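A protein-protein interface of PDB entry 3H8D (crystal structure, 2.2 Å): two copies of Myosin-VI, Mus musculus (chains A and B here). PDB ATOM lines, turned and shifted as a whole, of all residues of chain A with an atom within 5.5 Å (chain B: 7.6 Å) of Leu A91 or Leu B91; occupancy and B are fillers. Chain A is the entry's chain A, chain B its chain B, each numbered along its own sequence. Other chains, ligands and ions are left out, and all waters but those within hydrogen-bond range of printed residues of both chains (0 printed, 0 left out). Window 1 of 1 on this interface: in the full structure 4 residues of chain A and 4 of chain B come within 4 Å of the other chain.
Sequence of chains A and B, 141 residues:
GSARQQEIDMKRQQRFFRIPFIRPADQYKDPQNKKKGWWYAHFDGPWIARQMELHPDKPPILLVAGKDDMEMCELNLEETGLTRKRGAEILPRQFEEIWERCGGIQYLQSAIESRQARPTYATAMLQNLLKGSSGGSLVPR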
ATOM      1  N   PHE A  16      13.580 -18.859   1.923  1.00  0.00           N
ATOM      2  CA  PHE A  16      14.251 -18.369   3.123  1.00  0.00           C
ATOM      3  C   PHE A  16      14.050 -19.327   4.286  1.00  0.00           C
ATOM      4  O   PHE A  16      12.940 -19.796   4.528  1.00  0.00           O
ATOM      5  CB  PHE A  16      13.738 -16.967   3.472  1.00  0.00           C
ATOM      6  CG  PHE A  16      13.977 -15.950   2.384  1.00  0.00           C
ATOM      7  CD1 PHE A  16      15.141 -15.165   2.385  1.00  0.00           C
ATOM      8  CD2 PHE A  16      13.063 -15.792   1.341  1.00  0.00           C
ATOM      9  CE1 PHE A  16      15.377 -14.223   1.368  1.00  0.00           C
ATOM     10  CE2 PHE A  16      13.296 -14.864   0.311  1.00  0.00           C
ATOM     11  CZ  PHE A  16      14.452 -14.080   0.328  1.00  0.00           C
ATOM     12  N   GLU A  89      11.236 -22.933   7.347  1.00  0.00           N
ATOM     13  CA  GLU A  89      11.020 -21.896   6.327  1.00  0.00           C
ATOM     14  C   GLU A  89      10.458 -20.602   6.913  1.00  0.00           C
ATOM     15  O   GLU A  89       9.663 -20.624   7.848  1.00  0.00           O
ATOM     16  CB  GLU A  89      10.164 -22.402   5.150  1.00  0.00           C
ATOM     17  CG  GLU A  89      10.185 -21.417   3.965  1.00  0.00           C
ATOM     18  CD  GLU A  89       9.748 -21.979   2.625  1.00  0.00           C
ATOM     19  OE1 GLU A  89       9.270 -23.141   2.544  1.00  0.00           O
ATOM     20  OE2 GLU A  89       9.888 -21.222   1.633  1.00  0.00           O
ATOM     21  N   ILE A  90      10.888 -19.474   6.357  1.00  0.00           N
ATOM     22  CA  ILE A  90      10.449 -18.160   6.822  1.00  0.00           C
ATOM     23  C   ILE A  90      10.057 -17.280   5.643  1.00  0.00           C
ATOM     24  O   ILE A  90      10.424 -17.562   4.492  1.00  0.00           O
ATOM     25  CB  ILE A  90      11.531 -17.434   7.713  1.00  0.00           C
ATOM     26  CG1 ILE A  90      12.910 -17.439   7.045  1.00  0.00           C
ATOM     27  CG2 ILE A  90      11.614 -18.081   9.081  1.00  0.00           C
ATOM     28  CD1 ILE A  90      13.894 -16.404   7.609  1.00  0.00           C
ATOM     29  N   LEU A  91       9.313 -16.214   5.933  1.00  0.00           N
ATOM     30  CA  LEU A  91       8.959 -15.236   4.913  1.00  0.00           C
ATOM     31  C   LEU A  91      10.195 -14.419   4.526  1.00  0.00           C
ATOM     32  O   LEU A  91      11.101 -14.254   5.338  1.00  0.00           O
ATOM     33  CB  LEU A  91       7.803 -14.340   5.387  1.00  0.00           C
ATOM     34  CG  LEU A  91       6.444 -15.049   5.537  1.00  0.00           C
ATOM     35  CD1 LEU A  91       5.513 -14.257   6.450  1.00  0.00           C
ATOM     36  CD2 LEU A  91       5.798 -15.299   4.183  1.00  0.00           C
ATOM     37  N   PRO A  92      10.262 -13.945   3.264  1.00  0.00           N
ATOM     38  CA  PRO A  92      11.369 -13.070   2.856  1.00  0.00           C
ATOM     39  C   PRO A  92      11.661 -11.971   3.876  1.00  0.00           C
ATOM     40  O   PRO A  92      12.822 -11.738   4.201  1.00  0.00           O
ATOM     41  CB  PRO A  92      10.877 -12.466   1.528  1.00  0.00           C
ATOM     42  CG  PRO A  92      10.004 -13.532   0.941  1.00  0.00           C
ATOM     43  CD  PRO A  92       9.340 -14.237   2.144  1.00  0.00           C
ATOM     44  N   ARG A  93      10.611 -11.335   4.399  1.00  0.00           N
ATOM     45  CA  ARG A  93      10.752 -10.224   5.349  1.00  0.00           C
ATOM     46  C   ARG A  93      11.489 -10.585   6.646  1.00  0.00           C
ATOM     47  O   ARG A  93      12.255  -9.782   7.170  1.00  0.00           O
ATOM     48  CB  ARG A  93       9.376  -9.611   5.673  1.00  0.00           C
ATOM     49  CG  ARG A  93       9.439  -8.130   6.099  1.00  0.00           C
ATOM     50  CD  ARG A  93      10.004  -7.260   4.962  1.00  0.00           C
ATOM     51  NE  ARG A  93      11.094  -6.376   5.394  1.00  0.00           N
ATOM     52  CZ  ARG A  93      12.035  -5.887   4.584  1.00  0.00           C
ATOM     53  NH1 ARG A  93      12.984  -5.098   5.075  1.00  0.00           N
ATOM     54  NH2 ARG A  93      12.037  -6.186   3.287  1.00  0.00           N
ATOM     55  N   GLN A  94      11.236 -11.786   7.156  1.00  0.00           N
ATOM     56  CA  GLN A  94      11.927 -12.315   8.324  1.00  0.00           C
ATOM     57  C   GLN A  94      13.445 -12.451   8.120  1.00  0.00           C
ATOM     58  O   GLN A  94      14.207 -12.365   9.085  1.00  0.00           O
ATOM     59  CB  GLN A  94      11.316 -13.655   8.736  1.00  0.00           C
ATOM     60  CG  GLN A  94       9.919 -13.521   9.344  1.00  0.00           C
ATOM     61  CD  GLN A  94       9.233 -14.856   9.565  1.00  0.00           C
ATOM     62  OE1 GLN A  94       8.865 -15.548   8.612  1.00  0.00           O
ATOM     63  NE2 GLN A  94       9.045 -15.222  10.827  1.00  0.00           N
ATOM     64  N   PHE A  95      13.878 -12.667   6.877  1.00  0.00           N
ATOM     65  CA  PHE A  95      15.308 -12.687   6.551  1.00  0.00           C
ATOM     66  C   PHE A  95      15.841 -11.266   6.406  1.00  0.00           C
ATOM     67  O   PHE A  95      16.870 -10.920   6.992  1.00  0.00           O
ATOM     68  CB  PHE A  95      15.588 -13.492   5.270  1.00  0.00           C
ATOM     69  CG  PHE A  95      17.074 -13.679   4.956  1.00  0.00           C
ATOM     70  CD1 PHE A  95      17.717 -14.884   5.246  1.00  0.00           C
ATOM     71  CD2 PHE A  95      17.825 -12.648   4.385  1.00  0.00           C
ATOM     72  CE1 PHE A  95      19.094 -15.062   4.962  1.00  0.00           C
ATOM     73  CE2 PHE A  95      19.192 -12.813   4.099  1.00  0.00           C
ATOM     74  CZ  PHE A  95      19.828 -14.028   4.391  1.00  0.00           C
ATOM     75  N   GLN B  14       1.073 -14.313  -4.683  1.00  0.00           N
ATOM     76  CA  GLN B  14       0.148 -15.025  -3.834  1.00  0.00           C
ATOM     77  C   GLN B  14       0.524 -14.759  -2.370  1.00  0.00           C
ATOM     78  O   GLN B  14       1.674 -14.959  -1.979  1.00  0.00           O
ATOM     79  CB  GLN B  14       0.184 -16.524  -4.175  1.00  0.00           C
ATOM     80  CG  GLN B  14      -0.075 -16.844  -5.664  1.00  0.00           C
ATOM     81  CD  GLN B  14      -1.381 -16.254  -6.191  1.00  0.00           C
ATOM     82  OE1 GLN B  14      -2.464 -16.644  -5.771  1.00  0.00           O
ATOM     83  NE2 GLN B  14      -1.274 -15.302  -7.111  1.00  0.00           N
ATOM     84  N   ARG B  15      -0.423 -14.264  -1.573  1.00  0.00           N
ATOM     85  CA  ARG B  15      -0.146 -13.997  -0.146  1.00  0.00           C
ATOM     86  C   ARG B  15      -1.172 -14.632   0.791  1.00  0.00           C
ATOM     87  O   ARG B  15      -2.353 -14.718   0.465  1.00  0.00           O
ATOM     88  CB  ARG B  15       0.058 -12.502   0.121  1.00  0.00           C
ATOM     89  CG  ARG B  15       1.365 -11.986  -0.488  1.00  0.00           C
ATOM     90  CD  ARG B  15       1.542 -10.501  -0.345  1.00  0.00           C
ATOM     91  NE  ARG B  15       2.163 -10.199   0.936  1.00  0.00           N
ATOM     92  CZ  ARG B  15       2.619  -9.007   1.292  1.00  0.00           C
ATOM     93  NH1 ARG B  15       3.170  -8.848   2.487  1.00  0.00           N
ATOM     94  NH2 ARG B  15       2.528  -7.977   0.462  1.00  0.00           N
ATOM     95  N   PHE B  16      -0.687 -15.106   1.938  1.00  0.00           N
ATOM     96  CA  PHE B  16      -1.476 -15.907   2.881  1.00  0.00           C
ATOM     97  C   PHE B  16      -1.419 -15.270   4.264  1.00  0.00           C
ATOM     98  O   PHE B  16      -0.371 -14.769   4.687  1.00  0.00           O
ATOM     99  CB  PHE B  16      -0.990 -17.365   2.909  1.00  0.00           C
ATOM    100  CG  PHE B  16      -1.036 -18.038   1.563  1.00  0.00           C
ATOM    101  CD1 PHE B  16      -2.141 -18.784   1.183  1.00  0.00           C
ATOM    102  CD2 PHE B  16       0.008 -17.889   0.657  1.00  0.00           C
ATOM    103  CE1 PHE B  16      -2.191 -19.398  -0.064  1.00  0.00           C
ATOM    104  CE2 PHE B  16      -0.044 -18.489  -0.591  1.00  0.00           C
ATOM    105  CZ  PHE B  16      -1.148 -19.237  -0.952  1.00  0.00           C
ATOM    106  N   PHE B  17      -2.569 -15.255   4.938  1.00  0.00           N
ATOM    107  CA  PHE B  17      -2.716 -14.586   6.225  1.00  0.00           C
ATOM    108  C   PHE B  17      -3.500 -15.461   7.178  1.00  0.00           C
ATOM    109  O   PHE B  17      -4.337 -16.256   6.758  1.00  0.00           O
ATOM    110  CB  PHE B  17      -3.317 -13.175   6.062  1.00  0.00           C
ATOM    111  CG  PHE B  17      -2.506 -12.303   5.150  1.00  0.00           C
ATOM    112  CD1 PHE B  17      -2.765 -12.276   3.777  1.00  0.00           C
ATOM    113  CD2 PHE B  17      -1.456 -11.545   5.645  1.00  0.00           C
ATOM    114  CE1 PHE B  17      -1.989 -11.500   2.917  1.00  0.00           C
ATOM    115  CE2 PHE B  17      -0.671 -10.760   4.785  1.00  0.00           C
ATOM    116  CZ  PHE B  17      -0.938 -10.743   3.423  1.00  0.00           C
ATOM    117  N   ARG B  18      -3.159 -15.352   8.458  1.00  0.00           N
ATOM    118  CA  ARG B  18      -3.801 -16.133   9.498  1.00  0.00           C
ATOM    119  C   ARG B  18      -4.056 -15.251  10.710  1.00  0.00           C
ATOM    120  O   ARG B  18      -3.141 -14.601  11.212  1.00  0.00           O
ATOM    121  CB  ARG B  18      -2.941 -17.340   9.887  1.00  0.00           C
ATOM    122  CG  ARG B  18      -3.509 -18.154  11.079  1.00  0.00           C
ATOM    123  CD  ARG B  18      -2.547 -19.236  11.532  1.00  0.00           C
ATOM    124  NE  ARG B  18      -1.204 -18.707  11.791  1.00  0.00           N
ATOM    125  CZ  ARG B  18      -0.109 -19.449  11.901  1.00  0.00           C
ATOM    126  NH1 ARG B  18      -0.165 -20.763  11.747  1.00  0.00           N
ATOM    127  NH2 ARG B  18       1.057 -18.868  12.138  1.00  0.00           N
ATOM    128  N   GLY B  87       2.924 -10.759  12.344  1.00  0.00           N
ATOM    129  CA  GLY B  87       2.484 -12.117  12.662  1.00  0.00           C
ATOM    130  C   GLY B  87       1.341 -12.674  11.832  1.00  0.00           C
ATOM    131  O   GLY B  87       1.115 -13.885  11.832  1.00  0.00           O
ATOM    132  N   ALA B  88       0.619 -11.807  11.130  1.00  0.00           N
ATOM    133  CA  ALA B  88      -0.532 -12.242  10.329  1.00  0.00           C
ATOM    134  C   ALA B  88      -0.149 -13.067   9.098  1.00  0.00           C
ATOM    135  O   ALA B  88      -0.789 -14.080   8.800  1.00  0.00           O
ATOM    136  CB  ALA B  88      -1.409 -11.050   9.929  1.00  0.00           C
ATOM    137  N   GLU B  89       0.905 -12.648   8.400  1.00  0.00           N
ATOM    138  CA  GLU B  89       1.319 -13.321   7.177  1.00  0.00           C
ATOM    139  C   GLU B  89       1.930 -14.691   7.450  1.00  0.00           C
ATOM    140  O   GLU B  89       2.715 -14.876   8.379  1.00  0.00           O
ATOM    141  CB  GLU B  89       2.258 -12.455   6.314  1.00  0.00           C
ATOM    142  CG  GLU B  89       2.369 -12.989   4.875  1.00  0.00           C
ATOM    143  CD  GLU B  89       3.051 -12.046   3.891  1.00  0.00           C
ATOM    144  OE1 GLU B  89       3.409 -10.928   4.283  1.00  0.00           O
ATOM    145  OE2 GLU B  89       3.233 -12.432   2.714  1.00  0.00           O
ATOM    146  N   ILE B  90       1.537 -15.649   6.624  1.00  0.00           N
ATOM    147  CA  ILE B  90       2.038 -17.007   6.709  1.00  0.00           C
ATOM    148  C   ILE B  90       2.562 -17.463   5.346  1.00  0.00           C
ATOM    149  O   ILE B  90       2.289 -16.836   4.308  1.00  0.00           O
ATOM    150  CB  ILE B  90       0.954 -18.010   7.255  1.00  0.00           C
ATOM    151  CG1 ILE B  90      -0.402 -17.820   6.567  1.00  0.00           C
ATOM    152  CG2 ILE B  90       0.840 -17.904   8.770  1.00  0.00           C
ATOM    153  CD1 ILE B  90      -1.395 -19.016   6.705  1.00  0.00           C
ATOM    154  N   LEU B  91       3.311 -18.555   5.370  1.00  0.00           N
ATOM    155  CA  LEU B  91       3.790 -19.219   4.163  1.00  0.00           C
ATOM    156  C   LEU B  91       2.668 -20.033   3.500  1.00  0.00           C
ATOM    157  O   LEU B  91       1.709 -20.434   4.183  1.00  0.00           O
ATOM    158  CB  LEU B  91       4.987 -20.114   4.509  1.00  0.00           C
ATOM    159  CG  LEU B  91       6.260 -19.328   4.865  1.00  0.00           C
ATOM    160  CD1 LEU B  91       7.152 -20.142   5.780  1.00  0.00           C
ATOM    161  CD2 LEU B  91       7.015 -18.906   3.621  1.00  0.00           C
ATOM    162  N   PRO B  92       2.769 -20.262   2.164  1.00  0.00           N
ATOM    163  CA  PRO B  92       1.778 -21.084   1.458  1.00  0.00           C
ATOM    164  C   PRO B  92       1.429 -22.410   2.138  1.00  0.00           C
ATOM    165  O   PRO B  92       0.250 -22.738   2.248  1.00  0.00           O
ATOM    166  CB  PRO B  92       2.417 -21.302   0.075  1.00  0.00           C
ATOM    167  CG  PRO B  92       3.236 -20.054  -0.145  1.00  0.00           C
ATOM    168  CD  PRO B  92       3.770 -19.694   1.237  1.00  0.00           C
ATOM    169  N   ARG B  93       2.426 -23.147   2.626  1.00  0.00           N
ATOM    170  CA  ARG B  93       2.172 -24.455   3.245  1.00  0.00           C
ATOM    171  C   ARG B  93       1.373 -24.366   4.553  1.00  0.00           C
ATOM    172  O   ARG B  93       0.577 -25.258   4.861  1.00  0.00           O
ATOM    173  CB  ARG B  93       3.483 -25.233   3.441  1.00  0.00           C
ATOM    174  CG  ARG B  93       3.326 -26.704   3.921  1.00  0.00           C
ATOM    175  CD  ARG B  93       2.513 -27.527   2.931  1.00  0.00           C
ATOM    176  NE  ARG B  93       2.122 -28.833   3.468  1.00  0.00           N
ATOM    177  CZ  ARG B  93       1.056 -29.524   3.055  1.00  0.00           C
ATOM    178  NH1 ARG B  93       0.262 -29.024   2.115  1.00  0.00           N
ATOM    179  NH2 ARG B  93       0.773 -30.705   3.594  1.00  0.00           N
ATOM    180  N   GLN B  94       1.559 -23.287   5.314  1.00  0.00           N
ATOM    181  CA  GLN B  94       0.757 -23.081   6.516  1.00  0.00           C
ATOM    182  C   GLN B  94      -0.756 -22.913   6.212  1.00  0.00           C
ATOM    183  O   GLN B  94      -1.607 -23.286   7.038  1.00  0.00           O
ATOM    184  CB  GLN B  94       1.317 -21.936   7.355  1.00  0.00           C
ATOM    185  CG  GLN B  94       2.739 -22.178   7.873  1.00  0.00           C
ATOM    186  CD  GLN B  94       3.330 -20.945   8.508  1.00  0.00           C
ATOM    187  OE1 GLN B  94       3.654 -19.986   7.827  1.00  0.00           O
ATOM    188  NE2 GLN B  94       3.463 -20.958   9.834  1.00  0.00           N
ATOM    189  N   PHE B  95      -1.084 -22.375   5.034  1.00  0.00           N
ATOM    190  CA  PHE B  95      -2.476 -22.347   4.545  1.00  0.00           C
ATOM    191  C   PHE B  95      -2.882 -23.696   3.936  1.00  0.00           C
ATOM    192  O   PHE B  95      -3.950 -24.238   4.255  1.00  0.00           O
ATOM    193  CB  PHE B  95      -2.683 -21.213   3.521  1.00  0.00           C
ATOM    194  CG  PHE B  95      -4.117 -21.055   3.047  1.00  0.00           C
ATOM    195  CD1 PHE B  95      -4.922 -20.042   3.557  1.00  0.00           C
ATOM    196  CD2 PHE B  95      -4.658 -21.912   2.077  1.00  0.00           C
ATOM    197  CE1 PHE B  95      -6.248 -19.886   3.119  1.00  0.00           C
ATOM    198  CE2 PHE B  95      -5.984 -21.770   1.651  1.00  0.00           C
ATOM    199  CZ  PHE B  95      -6.776 -20.747   2.164  1.00  0.00           C
ATOM    200  N   GLU B  96      -2.028 -24.240   3.074  1.00  0.00           N
ATOM    201  CA  GLU B  96      -2.381 -25.431   2.284  1.00  0.00           C
ATOM    202  C   GLU B  96      -2.573 -26.709   3.099  1.00  0.00           C
ATOM    203  O   GLU B  96      -3.483 -27.490   2.809  1.00  0.00           O
ATOM    204  CB  GLU B  96      -1.399 -25.639   1.116  1.00  0.00           C
ATOM    205  CG  GLU B  96      -1.283 -24.432   0.157  1.00  0.00           C
ATOM    206  CD  GLU B  96      -2.512 -24.202  -0.703  1.00  0.00           C
ATOM    207  OE1 GLU B  96      -2.466 -23.270  -1.538  1.00  0.00           O
ATOM    208  OE2 GLU B  96      -3.514 -24.946  -0.562  1.00  0.00           O
ATOM    209  N   GLU B  97      -1.731 -26.919   4.113  1.00  0.00           N
ATOM    210  CA  GLU B  97      -1.828 -28.073   5.008  1.00  0.00           C
ATOM    211  C   GLU B  97      -3.225 -28.143   5.640  1.00  0.00           C
ATOM    212  O   GLU B  97      -3.844 -29.200   5.715  1.00  0.00           O
ATOM    213  CB  GLU B  97      -0.728 -28.016   6.096  1.00  0.00           C
ATOM    214  CG  GLU B  97      -0.836 -26.826   7.099  1.00  0.00           C
ATOM    215  CD  GLU B  97       0.378 -26.648   8.023  1.00  0.00           C
ATOM    216  OE1 GLU B  97       1.528 -26.604   7.524  1.00  0.00           O
ATOM    217  OE2 GLU B  97       0.178 -26.517   9.255  1.00  0.00           O
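O of Phe A16 sits at hydrogen-bond distance from N of Ile A90 (2.8 Å). NH1 of Arg B15 is in salt-bridge range of OE1 of Glu B89. The backbone NH (N) of Leu A91 is in hydrogen-bond range of the side-chain amide oxygen (OE1) of Gln A94, 2.8 Å away. N of Ile B90 sits at hydrogen-bond distance from O of Phe B16 (2.9 Å). The side-chain amide oxygen (OE1) of Gln B94 sits at hydrogen-bond distance from the backbone NH (N) of Leu B91 (2.9 Å).
Of the 8 printed residues of chain A, 3 touch a printed residue of chain B. Of the 16 printed residues of chain B, 3 touch a printed residue of chain A. Printed residues of chain B that touch a printed residue of chain A: Glu B89, Ile B90 and Leu B91.
Among the printed residues, merely in contact across the chains: Glu A89 with Leu B91, Leu A91 with Glu B89, Ile A90 with Leu B91, Leu A91 with Ile B90 and Leu A91 with Leu B91.
Printed residues of chain A within 4 Å of Glu B89: Leu A91 (3.5 Å). Of the printed residues of chain A, Ile B90 touches Leu A91 (3.8 Å). Printed residues of chain B within 4 Å of Glu A89: Leu B91 (3.3 Å). The nearest residue of chain A that does not touch Leu B91 is Pro A92 (5.4 Å). The nearest printed residue of chain A that does not touch Glu B89 is Gln A94 (6.2 Å).
Glu A89 touches Leu B91, and with the chains exchanged Leu A91 touches Glu B89. Ile A90 touches Leu B91, and with the chains exchanged Leu A91 touches Ile B90. Leu B91 touches its own counterpart, Leu A91. Of the 5 pairs that touch across the chains among the printed residues, 5 have their exchanged pair printed and touching as well.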
